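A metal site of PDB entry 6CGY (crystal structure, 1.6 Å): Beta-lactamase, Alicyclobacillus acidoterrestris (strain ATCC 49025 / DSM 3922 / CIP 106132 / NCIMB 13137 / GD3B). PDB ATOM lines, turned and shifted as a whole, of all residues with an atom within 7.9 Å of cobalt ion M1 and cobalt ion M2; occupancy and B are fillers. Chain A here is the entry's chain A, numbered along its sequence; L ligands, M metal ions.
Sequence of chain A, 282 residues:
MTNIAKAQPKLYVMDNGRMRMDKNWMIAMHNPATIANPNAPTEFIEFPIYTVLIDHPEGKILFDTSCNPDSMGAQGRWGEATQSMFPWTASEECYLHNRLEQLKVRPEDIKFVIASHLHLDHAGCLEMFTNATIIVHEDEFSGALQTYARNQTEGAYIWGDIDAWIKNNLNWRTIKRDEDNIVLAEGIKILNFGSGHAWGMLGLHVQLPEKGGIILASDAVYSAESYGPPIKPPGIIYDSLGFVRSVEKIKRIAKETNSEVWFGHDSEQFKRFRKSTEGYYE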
ATOM      1  N   MET A  19      -3.689 -21.676   2.724  1.00  0.00           N
ATOM      2  CA  MET A  19      -3.376 -22.833   3.543  1.00  0.00           C
ATOM      3  C   MET A  19      -4.694 -23.442   4.010  1.00  0.00           C
ATOM      4  O   MET A  19      -5.706 -22.754   4.154  1.00  0.00           O
ATOM      5  CB  MET A  19      -2.544 -22.407   4.768  1.00  0.00           C
ATOM      6  CG  MET A  19      -2.156 -23.496   5.720  1.00  0.00           C
ATOM      7  SD  MET A  19      -0.972 -22.884   6.956  1.00  0.00           S
ATOM      8  CE  MET A  19       0.343 -22.377   5.841  1.00  0.00           C
ATOM      9  N   MET A  21      -6.323 -26.195   7.066  1.00  0.00           N
ATOM     10  CA  MET A  21      -6.054 -26.925   8.290  1.00  0.00           C
ATOM     11  C   MET A  21      -7.341 -27.187   9.045  1.00  0.00           C
ATOM     12  O   MET A  21      -8.370 -26.587   8.742  1.00  0.00           O
ATOM     13  CB  MET A  21      -5.102 -26.140   9.197  1.00  0.00           C
ATOM     14  CG  MET A  21      -5.727 -24.926   9.876  1.00  0.00           C
ATOM     15  SD  MET A  21      -4.402 -24.003  10.693  1.00  0.00           S
ATOM     16  CE  MET A  21      -5.350 -22.634  11.370  1.00  0.00           C
ATOM     17  N   PHE A  47      -7.614 -20.640   4.337  1.00  0.00           N
ATOM     18  CA  PHE A  47      -7.389 -19.254   4.720  1.00  0.00           C
ATOM     19  C   PHE A  47      -6.208 -18.676   3.974  1.00  0.00           C
ATOM     20  O   PHE A  47      -5.381 -19.420   3.450  1.00  0.00           O
ATOM     21  CB  PHE A  47      -7.195 -19.151   6.239  1.00  0.00           C
ATOM     22  CG  PHE A  47      -6.101 -20.021   6.763  1.00  0.00           C
ATOM     23  CD1 PHE A  47      -4.810 -19.543   6.873  1.00  0.00           C
ATOM     24  CD2 PHE A  47      -6.368 -21.321   7.187  1.00  0.00           C
ATOM     25  CE1 PHE A  47      -3.812 -20.353   7.360  1.00  0.00           C
ATOM     26  CE2 PHE A  47      -5.366 -22.135   7.666  1.00  0.00           C
ATOM     27  CZ  PHE A  47      -4.081 -21.648   7.755  1.00  0.00           C
ATOM     28  N   PRO A  48      -6.119 -17.355   3.908  1.00  0.00           N
ATOM     29  CA  PRO A  48      -5.070 -16.736   3.116  1.00  0.00           C
ATOM     30  C   PRO A  48      -3.770 -16.539   3.905  1.00  0.00           C
ATOM     31  O   PRO A  48      -3.817 -16.352   5.126  1.00  0.00           O
ATOM     32  CB  PRO A  48      -5.664 -15.383   2.743  1.00  0.00           C
ATOM     33  CG  PRO A  48      -6.576 -15.055   3.864  1.00  0.00           C
ATOM     34  CD  PRO A  48      -7.053 -16.353   4.473  1.00  0.00           C
ATOM     35  N   ILE A  49      -2.665 -16.569   3.178  1.00  0.00           N
ATOM     36  CA  ILE A  49      -1.328 -16.206   3.669  1.00  0.00           C
ATOM     37  C   ILE A  49      -0.974 -14.943   2.920  1.00  0.00           C
ATOM     38  O   ILE A  49      -1.028 -14.922   1.694  1.00  0.00           O
ATOM     39  CB  ILE A  49      -0.291 -17.288   3.333  1.00  0.00           C
ATOM     40  CG1 ILE A  49      -0.719 -18.672   3.839  1.00  0.00           C
ATOM     41  CG2 ILE A  49       1.085 -16.904   3.848  1.00  0.00           C
ATOM     42  CD1 ILE A  49      -1.191 -18.714   5.272  1.00  0.00           C
ATOM     43  N   ASP A  64       5.960  -9.375   7.622  1.00  0.00           N
ATOM     44  CA  ASP A  64       5.892 -10.840   7.358  1.00  0.00           C
ATOM     45  C   ASP A  64       6.438 -11.196   5.979  1.00  0.00           C
ATOM     46  O   ASP A  64       6.693 -10.319   5.141  1.00  0.00           O
ATOM     47  CB  ASP A  64       4.471 -11.409   7.529  1.00  0.00           C
ATOM     48  CG  ASP A  64       4.083 -11.609   8.994  1.00  0.00           C
ATOM     49  OD1 ASP A  64       4.972 -11.635   9.872  1.00  0.00           O
ATOM     50  OD2 ASP A  64       2.858 -11.759   9.253  1.00  0.00           O
ATOM     51  N   SER A 116       6.538 -10.940  12.465  1.00  0.00           N
ATOM     52  CA  SER A 116       5.523 -10.903  13.507  1.00  0.00           C
ATOM     53  C   SER A 116       5.783 -12.014  14.487  1.00  0.00           C
ATOM     54  O   SER A 116       5.568 -11.850  15.701  1.00  0.00           O
ATOM     55  CB  SER A 116       4.110 -11.033  12.935  1.00  0.00           C
ATOM     56  OG  SER A 116       3.880 -12.276  12.268  1.00  0.00           O
ATOM     57  N   HIS A 117       6.176 -13.159  13.944  1.00  0.00           N
ATOM     58  CA  HIS A 117       6.681 -14.299  14.698  1.00  0.00           C
ATOM     59  C   HIS A 117       7.393 -15.203  13.710  1.00  0.00           C
ATOM     60  O   HIS A 117       7.469 -14.838  12.513  1.00  0.00           O
ATOM     61  CB  HIS A 117       5.581 -15.010  15.523  1.00  0.00           C
ATOM     62  CG  HIS A 117       4.432 -15.546  14.724  1.00  0.00           C
ATOM     63  ND1 HIS A 117       3.751 -14.815  13.786  1.00  0.00           N
ATOM     64  CD2 HIS A 117       3.786 -16.731  14.806  1.00  0.00           C
ATOM     65  CE1 HIS A 117       2.744 -15.526  13.316  1.00  0.00           C
ATOM     66  NE2 HIS A 117       2.746 -16.693  13.911  1.00  0.00           N
ATOM     67  N   LEU A 118       7.926 -16.326  14.153  1.00  0.00           N
ATOM     68  CA  LEU A 118       8.799 -17.135  13.295  1.00  0.00           C
ATOM     69  C   LEU A 118       8.175 -18.447  12.809  1.00  0.00           C
ATOM     70  O   LEU A 118       8.882 -19.359  12.383  1.00  0.00           O
ATOM     71  CB  LEU A 118      10.157 -17.386  13.966  1.00  0.00           C
ATOM     72  CG  LEU A 118      10.980 -16.109  14.164  1.00  0.00           C
ATOM     73  CD1 LEU A 118      12.264 -16.379  14.929  1.00  0.00           C
ATOM     74  CD2 LEU A 118      11.289 -15.387  12.842  1.00  0.00           C
ATOM     75  N   HIS A 119       6.838 -18.497  12.810  1.00  0.00           N
ATOM     76  CA  HIS A 119       6.101 -19.608  12.228  1.00  0.00           C
ATOM     77  C   HIS A 119       6.332 -19.754  10.720  1.00  0.00           C
ATOM     78  O   HIS A 119       6.648 -18.784  10.044  1.00  0.00           O
ATOM     79  CB  HIS A 119       4.611 -19.487  12.507  1.00  0.00           C
ATOM     80  CG  HIS A 119       4.219 -19.952  13.871  1.00  0.00           C
ATOM     81  ND1 HIS A 119       2.980 -19.720  14.425  1.00  0.00           N
ATOM     82  CD2 HIS A 119       4.916 -20.648  14.799  1.00  0.00           C
ATOM     83  CE1 HIS A 119       2.924 -20.264  15.629  1.00  0.00           C
ATOM     84  NE2 HIS A 119       4.098 -20.833  15.883  1.00  0.00           N
ATOM     85  N   LEU A 120       6.148 -20.975  10.258  1.00  0.00           N
ATOM     86  CA  LEU A 120       6.391 -21.401   8.884  1.00  0.00           C
ATOM     87  C   LEU A 120       5.780 -20.510   7.810  1.00  0.00           C
ATOM     88  O   LEU A 120       6.341 -20.364   6.715  1.00  0.00           O
ATOM     89  CB  LEU A 120       5.910 -22.848   8.706  1.00  0.00           C
ATOM     90  CG  LEU A 120       4.402 -23.178   8.760  1.00  0.00           C
ATOM     91  CD1 LEU A 120       4.171 -24.682   8.565  1.00  0.00           C
ATOM     92  CD2 LEU A 120       3.730 -22.740  10.048  1.00  0.00           C
ATOM     93  N   ASP A 121       4.637 -19.897   8.123  1.00  0.00           N
ATOM     94  CA  ASP A 121       3.889 -19.111   7.142  1.00  0.00           C
ATOM     95  C   ASP A 121       4.075 -17.592   7.266  1.00  0.00           C
ATOM     96  O   ASP A 121       3.407 -16.838   6.565  1.00  0.00           O
ATOM     97  CB  ASP A 121       2.398 -19.430   7.265  1.00  0.00           C
ATOM     98  CG  ASP A 121       1.867 -19.223   8.670  1.00  0.00           C
ATOM     99  OD1 ASP A 121       2.570 -19.589   9.651  1.00  0.00           O
ATOM    100  OD2 ASP A 121       0.753 -18.695   8.803  1.00  0.00           O
ATOM    101  N   HIS A 122       4.978 -17.153   8.155  1.00  0.00           N
ATOM    102  CA  HIS A 122       5.300 -15.724   8.317  1.00  0.00           C
ATOM    103  C   HIS A 122       6.788 -15.447   8.113  1.00  0.00           C
ATOM    104  O   HIS A 122       7.168 -14.355   7.713  1.00  0.00           O
ATOM    105  CB  HIS A 122       4.841 -15.231   9.684  1.00  0.00           C
ATOM    106  CG  HIS A 122       3.374 -15.432   9.908  1.00  0.00           C
ATOM    107  ND1 HIS A 122       2.453 -14.413   9.746  1.00  0.00           N
ATOM    108  CD2 HIS A 122       2.660 -16.539  10.202  1.00  0.00           C
ATOM    109  CE1 HIS A 122       1.235 -14.900   9.951  1.00  0.00           C
ATOM    110  NE2 HIS A 122       1.340 -16.181  10.221  1.00  0.00           N
ATOM    111  N   GLU A 140      10.968 -14.911  20.814  1.00  0.00           N
ATOM    112  CA  GLU A 140      10.565 -15.696  19.660  1.00  0.00           C
ATOM    113  C   GLU A 140      11.825 -16.213  18.929  1.00  0.00           C
ATOM    114  O   GLU A 140      11.892 -17.386  18.508  1.00  0.00           O
ATOM    115  CB  GLU A 140       9.662 -14.847  18.760  1.00  0.00           C
ATOM    116  CG  GLU A 140       9.165 -15.584  17.527  1.00  0.00           C
ATOM    117  CD  GLU A 140       8.100 -16.636  17.819  1.00  0.00           C
ATOM    118  OE1 GLU A 140       7.639 -16.736  18.971  1.00  0.00           O
ATOM    119  OE2 GLU A 140       7.694 -17.374  16.879  1.00  0.00           O
ATOM    120  N   ALA A 156       5.899 -26.164  13.538  1.00  0.00           N
ATOM    121  CA  ALA A 156       5.688 -24.832  12.963  1.00  0.00           C
ATOM    122  C   ALA A 156       6.948 -24.022  12.761  1.00  0.00           C
ATOM    123  O   ALA A 156       6.915 -22.976  12.124  1.00  0.00           O
ATOM    124  CB  ALA A 156       4.748 -24.038  13.854  1.00  0.00           C
ATOM    125  N   TYR A 157       8.057 -24.485  13.339  1.00  0.00           N
ATOM    126  CA  TYR A 157       9.328 -23.825  13.149  1.00  0.00           C
ATOM    127  C   TYR A 157      10.171 -24.684  12.225  1.00  0.00           C
ATOM    128  O   TYR A 157      10.510 -25.820  12.563  1.00  0.00           O
ATOM    129  CB  TYR A 157       9.977 -23.574  14.504  1.00  0.00           C
ATOM    130  CG  TYR A 157       9.197 -22.559  15.315  1.00  0.00           C
ATOM    131  CD1 TYR A 157       9.320 -21.189  15.064  1.00  0.00           C
ATOM    132  CD2 TYR A 157       8.314 -22.969  16.293  1.00  0.00           C
ATOM    133  CE1 TYR A 157       8.597 -20.269  15.794  1.00  0.00           C
ATOM    134  CE2 TYR A 157       7.564 -22.064  17.003  1.00  0.00           C
ATOM    135  CZ  TYR A 157       7.708 -20.716  16.750  1.00  0.00           C
ATOM    136  OH  TYR A 157       6.965 -19.813  17.465  1.00  0.00           O
ATOM    137  N   HIS A 197      -0.003 -16.318  21.251  1.00  0.00           N
ATOM    138  CA  HIS A 197      -0.002 -17.286  20.184  1.00  0.00           C
ATOM    139  C   HIS A 197       1.342 -18.012  20.073  1.00  0.00           C
ATOM    140  O   HIS A 197       1.379 -19.218  19.856  1.00  0.00           O
ATOM    141  CB  HIS A 197      -0.336 -16.559  18.874  1.00  0.00           C
ATOM    142  CG  HIS A 197      -0.110 -17.370  17.648  1.00  0.00           C
ATOM    143  ND1 HIS A 197      -0.924 -18.421  17.281  1.00  0.00           N
ATOM    144  CD2 HIS A 197       0.825 -17.272  16.665  1.00  0.00           C
ATOM    145  CE1 HIS A 197      -0.505 -18.927  16.140  1.00  0.00           C
ATOM    146  NE2 HIS A 197       0.556 -18.244  15.740  1.00  0.00           N
ATOM    147  N   ALA A 198       2.436 -17.279  20.225  1.00  0.00           N
ATOM    148  CA  ALA A 198       3.781 -17.833  20.199  1.00  0.00           C
ATOM    149  C   ALA A 198       4.603 -17.179  21.320  1.00  0.00           C
ATOM    150  O   ALA A 198       4.043 -16.517  22.194  1.00  0.00           O
ATOM    151  CB  ALA A 198       4.427 -17.574  18.824  1.00  0.00           C
ATOM    152  N   MET A 201       5.180 -12.020  20.038  1.00  0.00           N
ATOM    153  CA  MET A 201       4.416 -11.545  18.886  1.00  0.00           C
ATOM    154  C   MET A 201       4.635 -10.045  18.695  1.00  0.00           C
ATOM    155  O   MET A 201       4.469  -9.284  19.627  1.00  0.00           O
ATOM    156  CB  MET A 201       2.929 -11.789  19.085  1.00  0.00           C
ATOM    157  CG  MET A 201       2.540 -13.241  19.319  1.00  0.00           C
ATOM    158  SD  MET A 201       2.941 -14.334  17.950  1.00  0.00           S
ATOM    159  CE  MET A 201       1.869 -13.684  16.680  1.00  0.00           C
ATOM    160  N   SER A 218      -1.306  -9.801  12.660  1.00  0.00           N
ATOM    161  CA  SER A 218      -0.848 -11.163  12.362  1.00  0.00           C
ATOM    162  C   SER A 218      -1.608 -12.163  13.233  1.00  0.00           C
ATOM    163  O   SER A 218      -2.795 -11.986  13.502  1.00  0.00           O
ATOM    164  CB  SER A 218       0.667 -11.278  12.539  1.00  0.00           C
ATOM    165  OG  SER A 218       1.167 -12.561  12.145  1.00  0.00           O
ATOM    166  N   ASP A 219      -0.912 -13.187  13.701  1.00  0.00           N
ATOM    167  CA  ASP A 219      -1.559 -14.292  14.427  1.00  0.00           C
ATOM    168  C   ASP A 219      -1.884 -13.988  15.884  1.00  0.00           C
ATOM    169  O   ASP A 219      -2.370 -14.864  16.602  1.00  0.00           O
ATOM    170  CB  ASP A 219      -0.737 -15.570  14.290  1.00  0.00           C
ATOM    171  CG  ASP A 219      -0.755 -16.128  12.889  1.00  0.00           C
ATOM    172  OD1 ASP A 219      -1.431 -15.530  12.014  1.00  0.00           O
ATOM    173  OD2 ASP A 219      -0.113 -17.169  12.675  1.00  0.00           O
ATOM    174  N   ALA A 220      -1.671 -12.751  16.328  1.00  0.00           N
ATOM    175  CA  ALA A 220      -2.244 -12.352  17.605  1.00  0.00           C
ATOM    176  C   ALA A 220      -3.781 -12.398  17.515  1.00  0.00           C
ATOM    177  O   ALA A 220      -4.456 -12.599  18.536  1.00  0.00           O
ATOM    178  CB  ALA A 220      -1.742 -10.969  18.008  1.00  0.00           C
ATOM    179  N   TYR A 222      -6.307 -14.312  14.690  1.00  0.00           N
ATOM    180  CA  TYR A 222      -6.419 -15.035  13.439  1.00  0.00           C
ATOM    181  C   TYR A 222      -7.510 -14.483  12.541  1.00  0.00           C
ATOM    182  O   TYR A 222      -7.355 -14.403  11.314  1.00  0.00           O
ATOM    183  CB  TYR A 222      -6.763 -16.490  13.699  1.00  0.00           C
ATOM    184  CG  TYR A 222      -5.630 -17.480  13.929  1.00  0.00           C
ATOM    185  CD1 TYR A 222      -4.365 -17.313  13.377  1.00  0.00           C
ATOM    186  CD2 TYR A 222      -5.876 -18.627  14.664  1.00  0.00           C
ATOM    187  CE1 TYR A 222      -3.376 -18.269  13.557  1.00  0.00           C
ATOM    188  CE2 TYR A 222      -4.902 -19.579  14.833  1.00  0.00           C
ATOM    189  CZ  TYR A 222      -3.655 -19.414  14.285  1.00  0.00           C
ATOM    190  OH  TYR A 222      -2.715 -20.403  14.467  1.00  0.00           O
ATOM    191  N   GLY A 264      -4.615 -11.953  10.955  1.00  0.00           N
ATOM    192  CA  GLY A 264      -3.619 -12.799  10.315  1.00  0.00           C
ATOM    193  C   GLY A 264      -4.128 -13.614   9.154  1.00  0.00           C
ATOM    194  O   GLY A 264      -3.469 -13.715   8.122  1.00  0.00           O
ATOM    195  N   HIS A 265      -5.304 -14.223   9.321  1.00  0.00           N
ATOM    196  CA  HIS A 265      -5.756 -15.234   8.388  1.00  0.00           C
ATOM    197  C   HIS A 265      -7.298 -15.237   8.235  1.00  0.00           C
ATOM    198  O   HIS A 265      -7.932 -16.264   8.416  1.00  0.00           O
ATOM    199  CB  HIS A 265      -5.290 -16.614   8.855  1.00  0.00           C
ATOM    200  CG  HIS A 265      -3.786 -16.776   8.924  1.00  0.00           C
ATOM    201  ND1 HIS A 265      -2.966 -16.656   7.813  1.00  0.00           N
ATOM    202  CD2 HIS A 265      -2.978 -17.111   9.950  1.00  0.00           C
ATOM    203  CE1 HIS A 265      -1.719 -16.878   8.175  1.00  0.00           C
ATOM    204  NE2 HIS A 265      -1.698 -17.163   9.462  1.00  0.00           N
HETATM  205  P1  LIG L   1       0.230 -20.042  11.984  1.00  0.00           P
HETATM  206  O1  LIG L   1      -0.976 -19.509  11.235  1.00  0.00           O
HETATM  207  O2  LIG L   1       1.427 -19.096  11.748  1.00  0.00           O
HETATM  208  O3  LIG L   1      -0.057 -20.090  13.475  1.00  0.00           O
HETATM  209  O4  LIG L   1       0.514 -21.454  11.485  1.00  0.00           O
HETATM  210 CO    CO M   1       1.391 -18.402  13.782  1.00  0.00          CO
HETATM  211 CO    CO M   2      -0.044 -17.767  10.633  1.00  0.00          CO
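Cobalt ion M2 is bound by an oxygen (O1) of the ligand, a ring nitrogen (NE2) of His 265, the side-chain carboxylate of Asp 219, a ring nitrogen (NE2) of His 122, the side-chain carboxylate of Asp 121 and an oxygen (O2) of the ligand.
Cobalt ion M2 has six donor atoms within binding distance.
Of the 25 residues printed, 4 come within 4 Å of cobalt ion M1.
The nearest printed residue that does not touch cobalt ion M1 is His 122 (4.2 Å).
OG of Ser 218 lies close to ND1 of His 122, 3.3 Å away.
ND1 of His 117 lies within hydrogen-bond range of OG of Ser 116, 3.0 Å away.
The backbone carbonyl oxygen of Pro 48 is in hydrogen-bond range of a ring nitrogen (ND1) of His 265, 2.8 Å away.
The backbone NH (N) of His 265 lies within hydrogen-bond range of the backbone carbonyl oxygen (O) of Tyr 222.
OD2 of Asp 64 lies within hydrogen-bond range of ND1 of His 122 (2.7 Å).
OH of Tyr 157 is in hydrogen-bond range of NE2 of His 119, at 3.4 Å.
Cobalt ion M1 is bound by NE2 of His 197, O2 of the ligand, ND1 of His 119, NE2 of His 117, OD2 of Asp 219 and O3 of the ligand.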
